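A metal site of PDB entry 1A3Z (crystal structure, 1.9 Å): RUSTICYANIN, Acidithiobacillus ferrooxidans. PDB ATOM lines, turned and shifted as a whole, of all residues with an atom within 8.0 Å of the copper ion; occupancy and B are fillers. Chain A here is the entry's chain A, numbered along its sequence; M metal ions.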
ATOM      1  N   ALA A  44      31.613 -22.683  11.636  1.00  0.00           N
ATOM      2  CA  ALA A  44      30.195 -22.394  11.747  1.00  0.00           C
ATOM      3  C   ALA A  44      29.811 -21.323  10.731  1.00  0.00           C
ATOM      4  O   ALA A  44      30.136 -20.140  10.912  1.00  0.00           O
ATOM      5  CB  ALA A  44      29.866 -21.919  13.148  1.00  0.00           C
ATOM      6  N   VAL A  45      29.129 -21.750   9.673  1.00  0.00           N
ATOM      7  CA  VAL A  45      28.644 -20.880   8.591  1.00  0.00           C
ATOM      8  C   VAL A  45      29.714 -20.014   7.929  1.00  0.00           C
ATOM      9  O   VAL A  45      29.843 -18.839   8.237  1.00  0.00           O
ATOM     10  CB  VAL A  45      27.504 -19.953   9.089  1.00  0.00           C
ATOM     11  CG1 VAL A  45      26.800 -19.312   7.906  1.00  0.00           C
ATOM     12  CG2 VAL A  45      26.510 -20.756   9.919  1.00  0.00           C
ATOM     13  N   PHE A  51      22.568 -20.764   6.116  1.00  0.00           N
ATOM     14  CA  PHE A  51      22.502 -20.589   7.560  1.00  0.00           C
ATOM     15  C   PHE A  51      21.256 -21.313   8.063  1.00  0.00           C
ATOM     16  O   PHE A  51      20.188 -21.211   7.457  1.00  0.00           O
ATOM     17  CB  PHE A  51      22.391 -19.094   7.913  1.00  0.00           C
ATOM     18  CG  PHE A  51      22.057 -18.842   9.366  1.00  0.00           C
ATOM     19  CD1 PHE A  51      20.738 -18.941   9.827  1.00  0.00           C
ATOM     20  CD2 PHE A  51      23.064 -18.509  10.277  1.00  0.00           C
ATOM     21  CE1 PHE A  51      20.443 -18.724  11.178  1.00  0.00           C
ATOM     22  CE2 PHE A  51      22.766 -18.286  11.621  1.00  0.00           C
ATOM     23  CZ  PHE A  51      21.449 -18.395  12.073  1.00  0.00           C
ATOM     24  N   PRO A  52      21.395 -22.101   9.152  1.00  0.00           N
ATOM     25  CA  PRO A  52      22.634 -22.328   9.920  1.00  0.00           C
ATOM     26  C   PRO A  52      23.277 -23.633   9.478  1.00  0.00           C
ATOM     27  O   PRO A  52      22.579 -24.595   9.170  1.00  0.00           O
ATOM     28  CB  PRO A  52      22.132 -22.410  11.354  1.00  0.00           C
ATOM     29  CG  PRO A  52      20.706 -22.955  11.233  1.00  0.00           C
ATOM     30  CD  PRO A  52      20.247 -22.751   9.795  1.00  0.00           C
ATOM     31  N   SER A  53      24.606 -23.683   9.426  1.00  0.00           N
ATOM     32  CA  SER A  53      25.275 -24.896   9.007  1.00  0.00           C
ATOM     33  C   SER A  53      26.752 -24.986   9.419  1.00  0.00           C
ATOM     34  O   SER A  53      27.359 -23.989   9.798  1.00  0.00           O
ATOM     35  CB  SER A  53      25.141 -25.059   7.487  1.00  0.00           C
ATOM     36  OG  SER A  53      26.180 -24.382   6.793  1.00  0.00           O
ATOM     37  N   PHE A  54      27.306 -26.198   9.345  1.00  0.00           N
ATOM     38  CA  PHE A  54      28.712 -26.433   9.669  1.00  0.00           C
ATOM     39  C   PHE A  54      29.410 -26.725   8.345  1.00  0.00           C
ATOM     40  O   PHE A  54      28.826 -27.365   7.465  1.00  0.00           O
ATOM     41  CB  PHE A  54      28.871 -27.678  10.564  1.00  0.00           C
ATOM     42  CG  PHE A  54      28.479 -27.466  11.997  1.00  0.00           C
ATOM     43  CD1 PHE A  54      29.200 -26.620  12.817  1.00  0.00           C
ATOM     44  CD2 PHE A  54      27.362 -28.119  12.512  1.00  0.00           C
ATOM     45  CE1 PHE A  54      28.832 -26.418  14.149  1.00  0.00           C
ATOM     46  CE2 PHE A  54      26.971 -27.932  13.855  1.00  0.00           C
ATOM     47  CZ  PHE A  54      27.713 -27.085  14.668  1.00  0.00           C
ATOM     48  N   PHE A  76      37.550 -26.097  15.981  1.00  0.00           N
ATOM     49  CA  PHE A  76      36.294 -25.454  15.635  1.00  0.00           C
ATOM     50  C   PHE A  76      36.427 -23.923  15.586  1.00  0.00           C
ATOM     51  O   PHE A  76      36.879 -23.295  16.558  1.00  0.00           O
ATOM     52  CB  PHE A  76      35.213 -25.827  16.655  1.00  0.00           C
ATOM     53  CG  PHE A  76      33.911 -25.119  16.439  1.00  0.00           C
ATOM     54  CD1 PHE A  76      33.263 -25.183  15.212  1.00  0.00           C
ATOM     55  CD2 PHE A  76      33.329 -24.370  17.467  1.00  0.00           C
ATOM     56  CE1 PHE A  76      32.060 -24.531  15.014  1.00  0.00           C
ATOM     57  CE2 PHE A  76      32.119 -23.716  17.275  1.00  0.00           C
ATOM     58  CZ  PHE A  76      31.489 -23.791  16.044  1.00  0.00           C
ATOM     59  N   ASN A  78      34.263 -20.315  14.753  1.00  0.00           N
ATOM     60  CA  ASN A  78      32.976 -19.661  14.514  1.00  0.00           C
ATOM     61  C   ASN A  78      33.170 -18.419  13.632  1.00  0.00           C
ATOM     62  O   ASN A  78      33.543 -17.363  14.140  1.00  0.00           O
ATOM     63  CB  ASN A  78      32.313 -19.238  15.819  1.00  0.00           C
ATOM     64  CG  ASN A  78      31.018 -18.514  15.586  1.00  0.00           C
ATOM     65  OD1 ASN A  78      30.491 -18.546  14.466  1.00  0.00           O
ATOM     66  ND2 ASN A  78      30.505 -17.839  16.604  1.00  0.00           N
ATOM     67  N   ASN A  80      30.703 -17.047  11.901  1.00  0.00           N
ATOM     68  CA  ASN A  80      29.389 -16.454  11.691  1.00  0.00           C
ATOM     69  C   ASN A  80      29.129 -15.263  12.578  1.00  0.00           C
ATOM     70  O   ASN A  80      28.978 -15.397  13.792  1.00  0.00           O
ATOM     71  CB  ASN A  80      28.303 -17.507  11.930  1.00  0.00           C
ATOM     72  CG  ASN A  80      26.969 -17.109  11.348  1.00  0.00           C
ATOM     73  OD1 ASN A  80      25.917 -17.366  11.941  1.00  0.00           O
ATOM     74  ND2 ASN A  80      26.991 -16.473  10.183  1.00  0.00           N
ATOM     75  N   PHE A  83      26.299 -14.700  15.958  1.00  0.00           N
ATOM     76  CA  PHE A  83      25.902 -15.923  16.673  1.00  0.00           C
ATOM     77  C   PHE A  83      27.067 -16.711  17.245  1.00  0.00           C
ATOM     78  O   PHE A  83      28.124 -16.835  16.624  1.00  0.00           O
ATOM     79  CB  PHE A  83      25.086 -16.834  15.746  1.00  0.00           C
ATOM     80  CG  PHE A  83      23.829 -16.207  15.236  1.00  0.00           C
ATOM     81  CD1 PHE A  83      22.658 -16.237  15.989  1.00  0.00           C
ATOM     82  CD2 PHE A  83      23.816 -15.544  14.012  1.00  0.00           C
ATOM     83  CE1 PHE A  83      21.497 -15.617  15.538  1.00  0.00           C
ATOM     84  CE2 PHE A  83      22.652 -14.918  13.554  1.00  0.00           C
ATOM     85  CZ  PHE A  83      21.501 -14.955  14.320  1.00  0.00           C
ATOM     86  N   GLY A  84      26.851 -17.255  18.439  1.00  0.00           N
ATOM     87  CA  GLY A  84      27.879 -18.040  19.105  1.00  0.00           C
ATOM     88  C   GLY A  84      27.570 -19.524  19.025  1.00  0.00           C
ATOM     89  O   GLY A  84      27.258 -20.172  20.027  1.00  0.00           O
ATOM     90  N   HIS A  85      27.671 -20.070  17.823  1.00  0.00           N
ATOM     91  CA  HIS A  85      27.406 -21.490  17.597  1.00  0.00           C
ATOM     92  C   HIS A  85      28.278 -22.378  18.470  1.00  0.00           C
ATOM     93  O   HIS A  85      29.346 -21.955  18.904  1.00  0.00           O
ATOM     94  CB  HIS A  85      27.664 -21.838  16.127  1.00  0.00           C
ATOM     95  CG  HIS A  85      26.955 -20.946  15.154  1.00  0.00           C
ATOM     96  ND1 HIS A  85      25.595 -21.033  14.928  1.00  0.00           N
ATOM     97  CD2 HIS A  85      27.417 -20.001  14.302  1.00  0.00           C
ATOM     98  CE1 HIS A  85      25.253 -20.178  13.988  1.00  0.00           C
ATOM     99  NE2 HIS A  85      26.342 -19.543  13.581  1.00  0.00           N
ATOM    100  N   SER A  86      27.830 -23.603  18.711  1.00  0.00           N
ATOM    101  CA  SER A  86      28.605 -24.569  19.482  1.00  0.00           C
ATOM    102  C   SER A  86      28.848 -25.782  18.584  1.00  0.00           C
ATOM    103  O   SER A  86      28.242 -25.904  17.524  1.00  0.00           O
ATOM    104  CB  SER A  86      27.850 -25.010  20.749  1.00  0.00           C
ATOM    105  OG  SER A  86      26.790 -25.889  20.444  1.00  0.00           O
ATOM    106  N   PHE A  87      29.760 -26.648  18.988  1.00  0.00           N
ATOM    107  CA  PHE A  87      30.063 -27.860  18.217  1.00  0.00           C
ATOM    108  C   PHE A  87      30.145 -28.999  19.234  1.00  0.00           C
ATOM    109  O   PHE A  87      31.197 -29.234  19.834  1.00  0.00           O
ATOM    110  CB  PHE A  87      31.381 -27.704  17.472  1.00  0.00           C
ATOM    111  CG  PHE A  87      31.712 -28.865  16.577  1.00  0.00           C
ATOM    112  CD1 PHE A  87      32.315 -30.025  17.101  1.00  0.00           C
ATOM    113  CD2 PHE A  87      31.490 -28.787  15.200  1.00  0.00           C
ATOM    114  CE1 PHE A  87      32.685 -31.075  16.253  1.00  0.00           C
ATOM    115  CE2 PHE A  87      31.859 -29.838  14.351  1.00  0.00           C
ATOM    116  CZ  PHE A  87      32.460 -30.988  14.885  1.00  0.00           C
ATOM    117  N   PHE A 111      29.109 -22.941  23.907  1.00  0.00           N
ATOM    118  CA  PHE A 111      28.864 -21.773  23.057  1.00  0.00           C
ATOM    119  C   PHE A 111      30.116 -20.916  22.854  1.00  0.00           C
ATOM    120  O   PHE A 111      30.807 -20.574  23.796  1.00  0.00           O
ATOM    121  CB  PHE A 111      27.745 -20.939  23.660  1.00  0.00           C
ATOM    122  CG  PHE A 111      26.465 -21.681  23.805  1.00  0.00           C
ATOM    123  CD1 PHE A 111      25.896 -22.337  22.713  1.00  0.00           C
ATOM    124  CD2 PHE A 111      25.811 -21.735  25.030  1.00  0.00           C
ATOM    125  CE1 PHE A 111      24.703 -23.030  22.844  1.00  0.00           C
ATOM    126  CE2 PHE A 111      24.611 -22.425  25.167  1.00  0.00           C
ATOM    127  CZ  PHE A 111      24.054 -23.076  24.072  1.00  0.00           C
ATOM    128  N   VAL A 137      26.442 -31.486  16.590  1.00  0.00           N
ATOM    129  CA  VAL A 137      25.363 -30.517  16.515  1.00  0.00           C
ATOM    130  C   VAL A 137      25.630 -29.195  17.251  1.00  0.00           C
ATOM    131  O   VAL A 137      26.483 -29.124  18.142  1.00  0.00           O
ATOM    132  CB  VAL A 137      24.053 -31.126  17.101  1.00  0.00           C
ATOM    133  CG1 VAL A 137      23.961 -32.593  16.728  1.00  0.00           C
ATOM    134  CG2 VAL A 137      24.033 -30.987  18.605  1.00  0.00           C
ATOM    135  N   CYS A 138      24.886 -28.162  16.880  1.00  0.00           N
ATOM    136  CA  CYS A 138      24.999 -26.883  17.557  1.00  0.00           C
ATOM    137  C   CYS A 138      23.793 -26.793  18.480  1.00  0.00           C
ATOM    138  O   CYS A 138      22.670 -27.047  18.060  1.00  0.00           O
ATOM    139  CB  CYS A 138      24.965 -25.728  16.543  1.00  0.00           C
ATOM    140  SG  CYS A 138      24.794 -24.112  17.354  1.00  0.00           S
ATOM    141  N   GLN A 139      24.016 -26.427  19.742  1.00  0.00           N
ATOM    142  CA  GLN A 139      22.917 -26.334  20.715  1.00  0.00           C
ATOM    143  C   GLN A 139      22.139 -25.034  20.816  1.00  0.00           C
ATOM    144  O   GLN A 139      21.309 -24.880  21.714  1.00  0.00           O
ATOM    145  CB  GLN A 139      23.425 -26.676  22.113  1.00  0.00           C
ATOM    146  CG  GLN A 139      24.112 -28.023  22.223  1.00  0.00           C
ATOM    147  CD  GLN A 139      24.371 -28.395  23.656  1.00  0.00           C
ATOM    148  OE1 GLN A 139      23.424 -28.619  24.434  1.00  0.00           O
ATOM    149  NE2 GLN A 139      25.649 -28.453  24.035  1.00  0.00           N
ATOM    150  N   ILE A 140      22.408 -24.073  19.928  1.00  0.00           N
ATOM    151  CA  ILE A 140      21.652 -22.829  20.000  1.00  0.00           C
ATOM    152  C   ILE A 140      20.220 -23.167  19.599  1.00  0.00           C
ATOM    153  O   ILE A 140      19.973 -23.715  18.529  1.00  0.00           O
ATOM    154  CB  ILE A 140      22.187 -21.754  19.042  1.00  0.00           C
ATOM    155  CG1 ILE A 140      23.590 -21.314  19.473  1.00  0.00           C
ATOM    156  CG2 ILE A 140      21.231 -20.554  19.046  1.00  0.00           C
ATOM    157  CD1 ILE A 140      24.210 -20.300  18.536  1.00  0.00           C
ATOM    158  N   PRO A 141      19.255 -22.858  20.468  1.00  0.00           N
ATOM    159  CA  PRO A 141      17.853 -23.140  20.182  1.00  0.00           C
ATOM    160  C   PRO A 141      17.416 -22.921  18.732  1.00  0.00           C
ATOM    161  O   PRO A 141      17.607 -21.839  18.161  1.00  0.00           O
ATOM    162  CB  PRO A 141      17.108 -22.249  21.170  1.00  0.00           C
ATOM    163  CG  PRO A 141      18.025 -22.157  22.337  1.00  0.00           C
ATOM    164  CD  PRO A 141      19.433 -22.211  21.776  1.00  0.00           C
ATOM    165  N   GLY A 142      16.848 -23.957  18.151  1.00  0.00           N
ATOM    166  CA  GLY A 142      16.369 -23.879  16.783  1.00  0.00           C
ATOM    167  C   GLY A 142      17.382 -24.226  15.722  1.00  0.00           C
ATOM    168  O   GLY A 142      17.007 -24.578  14.612  1.00  0.00           O
ATOM    169  N   HIS A 143      18.669 -24.149  16.029  1.00  0.00           N
ATOM    170  CA  HIS A 143      19.665 -24.442  15.021  1.00  0.00           C
ATOM    171  C   HIS A 143      19.709 -25.885  14.523  1.00  0.00           C
ATOM    172  O   HIS A 143      19.595 -26.120  13.319  1.00  0.00           O
ATOM    173  CB  HIS A 143      21.052 -24.010  15.522  1.00  0.00           C
ATOM    174  CG  HIS A 143      21.258 -22.535  15.476  1.00  0.00           C
ATOM    175  ND1 HIS A 143      22.507 -21.943  15.551  1.00  0.00           N
ATOM    176  CD2 HIS A 143      20.372 -21.515  15.353  1.00  0.00           C
ATOM    177  CE1 HIS A 143      22.378 -20.639  15.464  1.00  0.00           C
ATOM    178  NE2 HIS A 143      21.099 -20.341  15.340  1.00  0.00           N
ATOM    179  N   ALA A 144      19.861 -26.841  15.439  1.00  0.00           N
ATOM    180  CA  ALA A 144      19.899 -28.251  15.053  1.00  0.00           C
ATOM    181  C   ALA A 144      18.565 -28.585  14.403  1.00  0.00           C
ATOM    182  O   ALA A 144      18.514 -29.278  13.384  1.00  0.00           O
ATOM    183  CB  ALA A 144      20.127 -29.124  16.265  1.00  0.00           C
ATOM    184  N   THR A 146      16.822 -26.945  12.571  1.00  0.00           N
ATOM    185  CA  THR A 146      16.740 -26.515  11.187  1.00  0.00           C
ATOM    186  C   THR A 146      17.895 -26.996  10.321  1.00  0.00           C
ATOM    187  O   THR A 146      18.124 -26.452   9.246  1.00  0.00           O
ATOM    188  CB  THR A 146      16.646 -24.985  11.050  1.00  0.00           C
ATOM    189  OG1 THR A 146      17.945 -24.416  11.235  1.00  0.00           O
ATOM    190  CG2 THR A 146      15.686 -24.404  12.101  1.00  0.00           C
ATOM    191  N   MET A 148      21.441 -27.734  11.497  1.00  0.00           N
ATOM    192  CA  MET A 148      22.844 -27.553  11.852  1.00  0.00           C
ATOM    193  C   MET A 148      23.397 -28.760  12.608  1.00  0.00           C
ATOM    194  O   MET A 148      23.613 -28.725  13.819  1.00  0.00           O
ATOM    195  CB  MET A 148      23.057 -26.281  12.696  1.00  0.00           C
ATOM    196  CG  MET A 148      24.413 -25.650  12.465  1.00  0.00           C
ATOM    197  SD  MET A 148      24.683 -24.090  13.343  1.00  0.00           S
ATOM    198  CE  MET A 148      26.488 -24.028  13.287  1.00  0.00           C
HETATM  199 CU    CU M   1      24.311 -22.678  15.678  1.00  0.00          CU
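The backbone carbonyl oxygen (O) of His 143 lies within hydrogen-bond range of the side-chain hydroxyl (OG1) of Thr 146 (3.2 Å).
NE2 of His 85 lies within hydrogen-bond range of OD1 of Asn 80.
SG of Cys 138 sits close to N of Ile 140.
SG of Cys 138 sits close to N of Ser 86, 3.4 Å away.
Residues that only touch the copper ion: Ile 140 (3.7 Å).
Five residues have an atom within 4 Å of the copper ion: His 85, Cys 138, Ile 140, His 143 and Met 148.
The nearest printed residue that does not touch the copper ion is Ser 86 (4.7 Å).
ND1 of His 143 is bound to the copper ion, at 2.0 Å.
ND1 of His 85 binds the copper ion (2.2 Å).
SG of Cys 138 is bound to the copper ion (2.3 Å).
SD of Met 148 is bound to the copper ion, 2.8 Å away.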
